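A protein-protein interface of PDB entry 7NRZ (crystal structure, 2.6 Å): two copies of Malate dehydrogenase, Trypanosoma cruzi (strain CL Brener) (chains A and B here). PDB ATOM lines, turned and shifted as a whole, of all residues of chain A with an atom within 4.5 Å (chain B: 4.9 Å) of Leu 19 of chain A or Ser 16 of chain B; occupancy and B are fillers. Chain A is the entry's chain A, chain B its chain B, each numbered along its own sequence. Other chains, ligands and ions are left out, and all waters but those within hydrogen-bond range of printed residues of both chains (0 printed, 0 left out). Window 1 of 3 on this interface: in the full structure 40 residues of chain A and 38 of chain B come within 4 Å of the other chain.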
ATOM      1  N   GLN A  15     -21.896  16.221  27.158  1.00  0.00           N
ATOM      2  CA  GLN A  15     -20.531  16.742  27.205  1.00  0.00           C
ATOM      3  C   GLN A  15     -19.748  16.343  25.960  1.00  0.00           C
ATOM      4  O   GLN A  15     -19.132  17.192  25.303  1.00  0.00           O
ATOM      5  CB  GLN A  15     -19.821  16.257  28.470  1.00  0.00           C
ATOM      6  CG  GLN A  15     -20.376  16.860  29.751  1.00  0.00           C
ATOM      7  CD  GLN A  15     -19.348  16.953  30.861  1.00  0.00           C
ATOM      8  OE1 GLN A  15     -18.167  17.203  30.614  1.00  0.00           O
ATOM      9  NE2 GLN A  15     -19.796  16.755  32.096  1.00  0.00           N
ATOM     10  N   SER A  16     -19.761  15.056  25.612  1.00  0.00           N
ATOM     11  CA  SER A  16     -19.038  14.621  24.424  1.00  0.00           C
ATOM     12  C   SER A  16     -19.684  15.178  23.158  1.00  0.00           C
ATOM     13  O   SER A  16     -18.983  15.580  22.221  1.00  0.00           O
ATOM     14  CB  SER A  16     -18.975  13.094  24.385  1.00  0.00           C
ATOM     15  OG  SER A  16     -18.105  12.601  25.392  1.00  0.00           O
ATOM     16  N   LEU A  17     -21.020  15.214  23.127  1.00  0.00           N
ATOM     17  CA  LEU A  17     -21.746  15.843  22.026  1.00  0.00           C
ATOM     18  C   LEU A  17     -21.310  17.289  21.840  1.00  0.00           C
ATOM     19  O   LEU A  17     -20.979  17.714  20.725  1.00  0.00           O
ATOM     20  CB  LEU A  17     -23.250  15.742  22.301  1.00  0.00           C
ATOM     21  CG  LEU A  17     -24.341  16.352  21.420  1.00  0.00           C
ATOM     22  CD1 LEU A  17     -23.957  16.338  19.971  1.00  0.00           C
ATOM     23  CD2 LEU A  17     -25.641  15.570  21.620  1.00  0.00           C
ATOM     24  N   SER A  18     -21.282  18.056  22.932  1.00  0.00           N
ATOM     25  CA  SER A  18     -20.849  19.447  22.860  1.00  0.00           C
ATOM     26  C   SER A  18     -19.403  19.556  22.393  1.00  0.00           C
ATOM     27  O   SER A  18     -19.058  20.457  21.619  1.00  0.00           O
ATOM     28  CB  SER A  18     -21.030  20.106  24.226  1.00  0.00           C
ATOM     29  OG  SER A  18     -22.387  20.038  24.634  1.00  0.00           O
ATOM     30  N   LEU A  19     -18.543  18.641  22.849  1.00  0.00           N
ATOM     31  CA  LEU A  19     -17.145  18.647  22.427  1.00  0.00           C
ATOM     32  C   LEU A  19     -17.022  18.464  20.918  1.00  0.00           C
ATOM     33  O   LEU A  19     -16.260  19.178  20.253  1.00  0.00           O
ATOM     34  CB  LEU A  19     -16.376  17.555  23.169  1.00  0.00           C
ATOM     35  CG  LEU A  19     -14.961  17.252  22.674  1.00  0.00           C
ATOM     36  CD1 LEU A  19     -14.066  18.479  22.799  1.00  0.00           C
ATOM     37  CD2 LEU A  19     -14.379  16.067  23.444  1.00  0.00           C
ATOM     38  N   LEU A  20     -17.766  17.507  20.357  1.00  0.00           N
ATOM     39  CA  LEU A  20     -17.718  17.298  18.915  1.00  0.00           C
ATOM     40  C   LEU A  20     -18.242  18.519  18.162  1.00  0.00           C
ATOM     41  O   LEU A  20     -17.647  18.940  17.160  1.00  0.00           O
ATOM     42  CB  LEU A  20     -18.507  16.044  18.535  1.00  0.00           C
ATOM     43  CG  LEU A  20     -17.984  14.711  19.083  1.00  0.00           C
ATOM     44  CD1 LEU A  20     -18.789  13.541  18.541  1.00  0.00           C
ATOM     45  CD2 LEU A  20     -16.507  14.530  18.779  1.00  0.00           C
ATOM     46  N   LEU A  21     -19.344  19.115  18.641  1.00  0.00           N
ATOM     47  CA  LEU A  21     -19.890  20.297  17.975  1.00  0.00           C
ATOM     48  C   LEU A  21     -18.902  21.454  18.006  1.00  0.00           C
ATOM     49  O   LEU A  21     -18.771  22.191  17.024  1.00  0.00           O
ATOM     50  CB  LEU A  21     -21.209  20.722  18.618  1.00  0.00           C
ATOM     51  CG  LEU A  21     -22.412  19.804  18.410  1.00  0.00           C
ATOM     52  CD1 LEU A  21     -23.649  20.421  19.023  1.00  0.00           C
ATOM     53  CD2 LEU A  21     -22.627  19.509  16.941  1.00  0.00           C
ATOM     54  N   LEU A  22     -18.199  21.631  19.127  1.00  0.00           N
ATOM     55  CA  LEU A  22     -17.195  22.688  19.202  1.00  0.00           C
ATOM     56  C   LEU A  22     -16.087  22.468  18.182  1.00  0.00           C
ATOM     57  O   LEU A  22     -15.599  23.423  17.566  1.00  0.00           O
ATOM     58  CB  LEU A  22     -16.606  22.763  20.608  1.00  0.00           C
ATOM     59  CG  LEU A  22     -15.510  23.824  20.736  1.00  0.00           C
ATOM     60  CD1 LEU A  22     -16.080  25.126  21.260  1.00  0.00           C
ATOM     61  CD2 LEU A  22     -14.374  23.338  21.600  1.00  0.00           C
ATOM     62  N   ARG A  23     -15.678  21.214  17.985  1.00  0.00           N
ATOM     63  CA  ARG A  23     -14.620  20.924  17.027  1.00  0.00           C
ATOM     64  C   ARG A  23     -15.091  21.095  15.590  1.00  0.00           C
ATOM     65  O   ARG A  23     -14.284  21.417  14.711  1.00  0.00           O
ATOM     66  CB  ARG A  23     -14.100  19.503  17.233  1.00  0.00           C
ATOM     67  CG  ARG A  23     -13.306  19.305  18.508  1.00  0.00           C
ATOM     68  CD  ARG A  23     -12.994  17.838  18.727  1.00  0.00           C
ATOM     69  NE  ARG A  23     -11.661  17.485  18.246  1.00  0.00           N
ATOM     70  CZ  ARG A  23     -11.417  16.891  17.083  1.00  0.00           C
ATOM     71  NH1 ARG A  23     -12.418  16.572  16.273  1.00  0.00           N
ATOM     72  NH2 ARG A  23     -10.170  16.610  16.733  1.00  0.00           N
ATOM     73  N   LEU A  46     -14.858  23.768  27.529  1.00  0.00           N
ATOM     74  CA  LEU A  46     -14.804  23.840  26.075  1.00  0.00           C
ATOM     75  C   LEU A  46     -14.263  25.180  25.595  1.00  0.00           C
ATOM     76  O   LEU A  46     -13.629  25.241  24.534  1.00  0.00           O
ATOM     77  CB  LEU A  46     -16.191  23.584  25.491  1.00  0.00           C
ATOM     78  CG  LEU A  46     -16.696  22.152  25.646  1.00  0.00           C
ATOM     79  CD1 LEU A  46     -18.160  22.065  25.249  1.00  0.00           C
ATOM     80  CD2 LEU A  46     -15.850  21.201  24.820  1.00  0.00           C
ATOM     81  N   ILE A  49     -10.531  25.457  24.509  1.00  0.00           N
ATOM     82  CA  ILE A  49     -10.020  24.865  23.283  1.00  0.00           C
ATOM     83  C   ILE A  49      -9.785  25.962  22.256  1.00  0.00           C
ATOM     84  O   ILE A  49     -10.539  26.943  22.180  1.00  0.00           O
ATOM     85  CB  ILE A  49     -10.994  23.787  22.779  1.00  0.00           C
ATOM     86  CG1 ILE A  49     -11.044  22.643  23.799  1.00  0.00           C
ATOM     87  CG2 ILE A  49     -10.587  23.279  21.396  1.00  0.00           C
ATOM     88  CD1 ILE A  49     -12.001  21.533  23.468  1.00  0.00           C
ATOM     89  N   GLY B  12     -13.256  10.139  32.896  1.00  0.00           N
ATOM     90  CA  GLY B  12     -13.834  11.259  32.170  1.00  0.00           C
ATOM     91  C   GLY B  12     -12.951  11.734  31.032  1.00  0.00           C
ATOM     92  O   GLY B  12     -13.434  11.990  29.926  1.00  0.00           O
ATOM     93  N   ILE B  13     -11.647  11.826  31.255  1.00  0.00           N
ATOM     94  CA  ILE B  13     -10.717  12.301  30.192  1.00  0.00           C
ATOM     95  C   ILE B  13     -10.563  11.201  29.152  1.00  0.00           C
ATOM     96  O   ILE B  13     -10.814  11.472  27.993  1.00  0.00           O
ATOM     97  CB  ILE B  13      -9.372  12.768  30.772  1.00  0.00           C
ATOM     98  CG1 ILE B  13      -9.548  13.889  31.795  1.00  0.00           C
ATOM     99  CG2 ILE B  13      -8.412  13.166  29.669  1.00  0.00           C
ATOM    100  CD1 ILE B  13      -8.511  13.894  32.880  1.00  0.00           C
ATOM    101  N   GLY B  14     -10.259   9.992  29.587  1.00  0.00           N
ATOM    102  CA  GLY B  14     -10.015   8.866  28.679  1.00  0.00           C
ATOM    103  C   GLY B  14     -11.145   8.589  27.728  1.00  0.00           C
ATOM    104  O   GLY B  14     -10.858   8.249  26.610  1.00  0.00           O
ATOM    105  N   GLN B  15     -12.377   8.683  28.190  1.00  0.00           N
ATOM    106  CA  GLN B  15     -13.498   8.368  27.305  1.00  0.00           C
ATOM    107  C   GLN B  15     -13.564   9.338  26.129  1.00  0.00           C
ATOM    108  O   GLN B  15     -13.630   8.917  24.967  1.00  0.00           O
ATOM    109  CB  GLN B  15     -14.812   8.370  28.090  1.00  0.00           C
ATOM    110  CG  GLN B  15     -14.992   7.156  28.990  1.00  0.00           C
ATOM    111  CD  GLN B  15     -16.453   6.829  29.263  1.00  0.00           C
ATOM    112  OE1 GLN B  15     -17.307   6.940  28.382  1.00  0.00           O
ATOM    113  NE2 GLN B  15     -16.743   6.414  30.491  1.00  0.00           N
ATOM    114  N   SER B  16     -13.547  10.645  26.408  1.00  0.00           N
ATOM    115  CA  SER B  16     -13.577  11.623  25.324  1.00  0.00           C
ATOM    116  C   SER B  16     -12.305  11.553  24.488  1.00  0.00           C
ATOM    117  O   SER B  16     -12.355  11.671  23.258  1.00  0.00           O
ATOM    118  CB  SER B  16     -13.779  13.030  25.887  1.00  0.00           C
ATOM    119  OG  SER B  16     -15.115  13.220  26.315  1.00  0.00           O
ATOM    120  N   LEU B  17     -11.160  11.359  25.145  1.00  0.00           N
ATOM    121  CA  LEU B  17      -9.897  11.162  24.440  1.00  0.00           C
ATOM    122  C   LEU B  17      -9.978   9.971  23.489  1.00  0.00           C
ATOM    123  O   LEU B  17      -9.571  10.060  22.323  1.00  0.00           O
ATOM    124  CB  LEU B  17      -8.774  10.984  25.470  1.00  0.00           C
ATOM    125  CG  LEU B  17      -7.281  10.919  25.129  1.00  0.00           C
ATOM    126  CD1 LEU B  17      -6.927  11.750  23.930  1.00  0.00           C
ATOM    127  CD2 LEU B  17      -6.461  11.375  26.332  1.00  0.00           C
ATOM    128  N   SER B  18     -10.510   8.847  23.970  1.00  0.00           N
ATOM    129  CA  SER B  18     -10.655   7.678  23.110  1.00  0.00           C
ATOM    130  C   SER B  18     -11.600   7.961  21.949  1.00  0.00           C
ATOM    131  O   SER B  18     -11.342   7.542  20.813  1.00  0.00           O
ATOM    132  CB  SER B  18     -11.138   6.484  23.933  1.00  0.00           C
ATOM    133  OG  SER B  18     -10.180   6.137  24.918  1.00  0.00           O
ATOM    134  N   LEU B  19     -12.697   8.681  22.214  1.00  0.00           N
ATOM    135  CA  LEU B  19     -13.635   9.031  21.152  1.00  0.00           C
ATOM    136  C   LEU B  19     -12.953   9.843  20.061  1.00  0.00           C
ATOM    137  O   LEU B  19     -13.155   9.585  18.869  1.00  0.00           O
ATOM    138  CB  LEU B  19     -14.824   9.798  21.731  1.00  0.00           C
ATOM    139  CG  LEU B  19     -15.744  10.531  20.745  1.00  0.00           C
ATOM    140  CD1 LEU B  19     -16.435   9.557  19.793  1.00  0.00           C
ATOM    141  CD2 LEU B  19     -16.773  11.371  21.497  1.00  0.00           C
ATOM    142  N   LEU B  20     -12.132  10.822  20.447  1.00  0.00           N
ATOM    143  CA  LEU B  20     -11.448  11.640  19.453  1.00  0.00           C
ATOM    144  C   LEU B  20     -10.469  10.805  18.632  1.00  0.00           C
ATOM    145  O   LEU B  20     -10.400  10.947  17.404  1.00  0.00           O
ATOM    146  CB  LEU B  20     -10.734  12.808  20.135  1.00  0.00           C
ATOM    147  CG  LEU B  20     -11.648  13.825  20.827  1.00  0.00           C
ATOM    148  CD1 LEU B  20     -10.851  14.982  21.402  1.00  0.00           C
ATOM    149  CD2 LEU B  20     -12.710  14.332  19.866  1.00  0.00           C
ATOM    150  N   LEU B 233     -12.873  17.771  28.866  1.00  0.00           N
ATOM    151  CA  LEU B 233     -13.078  17.843  27.424  1.00  0.00           C
ATOM    152  C   LEU B 233     -11.915  18.542  26.722  1.00  0.00           C
ATOM    153  O   LEU B 233     -11.423  18.051  25.699  1.00  0.00           O
ATOM    154  CB  LEU B 233     -14.403  18.543  27.126  1.00  0.00           C
ATOM    155  CG  LEU B 233     -15.619  17.937  27.839  1.00  0.00           C
ATOM    156  CD1 LEU B 233     -16.863  18.795  27.643  1.00  0.00           C
ATOM    157  CD2 LEU B 233     -15.875  16.506  27.371  1.00  0.00           C
ATOM    158  N   ALA B 236      -9.002  16.207  26.971  1.00  0.00           N
ATOM    159  CA  ALA B 236      -9.067  15.165  25.952  1.00  0.00           C
ATOM    160  C   ALA B 236      -8.653  15.699  24.587  1.00  0.00           C
ATOM    161  O   ALA B 236      -7.971  15.005  23.824  1.00  0.00           O
ATOM    162  CB  ALA B 236     -10.474  14.576  25.895  1.00  0.00           C
ATOM    163  N   GLU B 237      -9.057  16.928  24.260  1.00  0.00           N
ATOM    164  CA  GLU B 237      -8.681  17.517  22.978  1.00  0.00           C
ATOM    165  C   GLU B 237      -7.165  17.604  22.841  1.00  0.00           C
ATOM    166  O   GLU B 237      -6.600  17.245  21.801  1.00  0.00           O
ATOM    167  CB  GLU B 237      -9.319  18.900  22.833  1.00  0.00           C
ATOM    168  CG  GLU B 237      -8.822  19.696  21.639  1.00  0.00           C
ATOM    169  CD  GLU B 237      -9.279  19.121  20.317  1.00  0.00           C
ATOM    170  OE1 GLU B 237     -10.125  18.204  20.319  1.00  0.00           O
ATOM    171  OE2 GLU B 237      -8.788  19.583  19.269  1.00  0.00           O
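Ser 16 of chain A touches its own counterpart, Ser 16 of chain B.
Leu 19 of chain A touches Ser 16 of chain B, but with the chains exchanged Ser 16 of chain A does not touch Leu 19 of chain B (4.02 Å).
Leu 20 of chain B touches its own counterpart, Leu 20 of chain A.
Positions printed for both chains: 15, 16, 17, 18, 19 and 20.
Of the 9 pairs that touch across the chains among the printed residues, 2 have their exchanged pair printed and touching as well.
Leu 19 of chain A touches two residues of chain B.
Ser 16 of chain B touches just these residues of chain A: Ser 16 (3.2 Å) and Leu 19 (3.9 Å).
Printed residues of chain A within 4 Å of Glu 237 of chain B: Arg 23 (2.7 Å) and Ile 49 (3.8 Å).
Printed residues of chain B within 4 Å of Ser 16 of chain A: Ser 16 (3.2 Å).
Printed residues of chain A within 4 Å of Leu 20 of chain B: Leu 20 and Arg 23.
Printed residues of chain B within 4 Å of Ile 49 of chain A: Glu 237.
Ser 18 of chain A touches none of the printed residues of chain B.
Ile 13 of chain B touches none of the printed residues of chain A.
Of the 11 printed residues of chain A, 7 touch a printed residue of chain B.
Printed residues of chain A that touch a printed residue of chain B: Gln 15, Ser 16, Leu 19, Leu 20, Arg 23, Leu 46 and Ile 49.
Hydrophobic or aromatic side chains of chain A that line the printed part of chain B: Leu 19, Leu 20, Leu 46 and Ile 49.
Of the 12 printed residues of chain B, 4 touch a printed residue of chain A.
Among the printed residues, Asp or Glu carboxylates within 4 Å of a Lys or Arg side-chain nitrogen of the other chain: Arg 23 of chain A with Glu 237 of chain B.
OG of Ser 16 of chain A lies within hydrogen-bond range of OG of Ser 16 of chain B (3.2 Å).
NE of Arg 23 of chain A lies within salt-bridge range of OE1 of Glu 237 of chain B (2.7 Å).
Among the printed residues, pairs that only touch across the chains: Gln 15 of chain A with Leu 233 of chain B, Arg 23 of chain A with Leu 20 of chain B, Leu 46 of chain A with Leu 233 of chain B, Ile 49 of chain A with Glu 237 of chain B, Leu 19 of chain A with Ser 16 of chain B, Leu 19 of chain A with Leu 233 of chain B and Leu 20 of chain A with Leu 20 of chain B.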
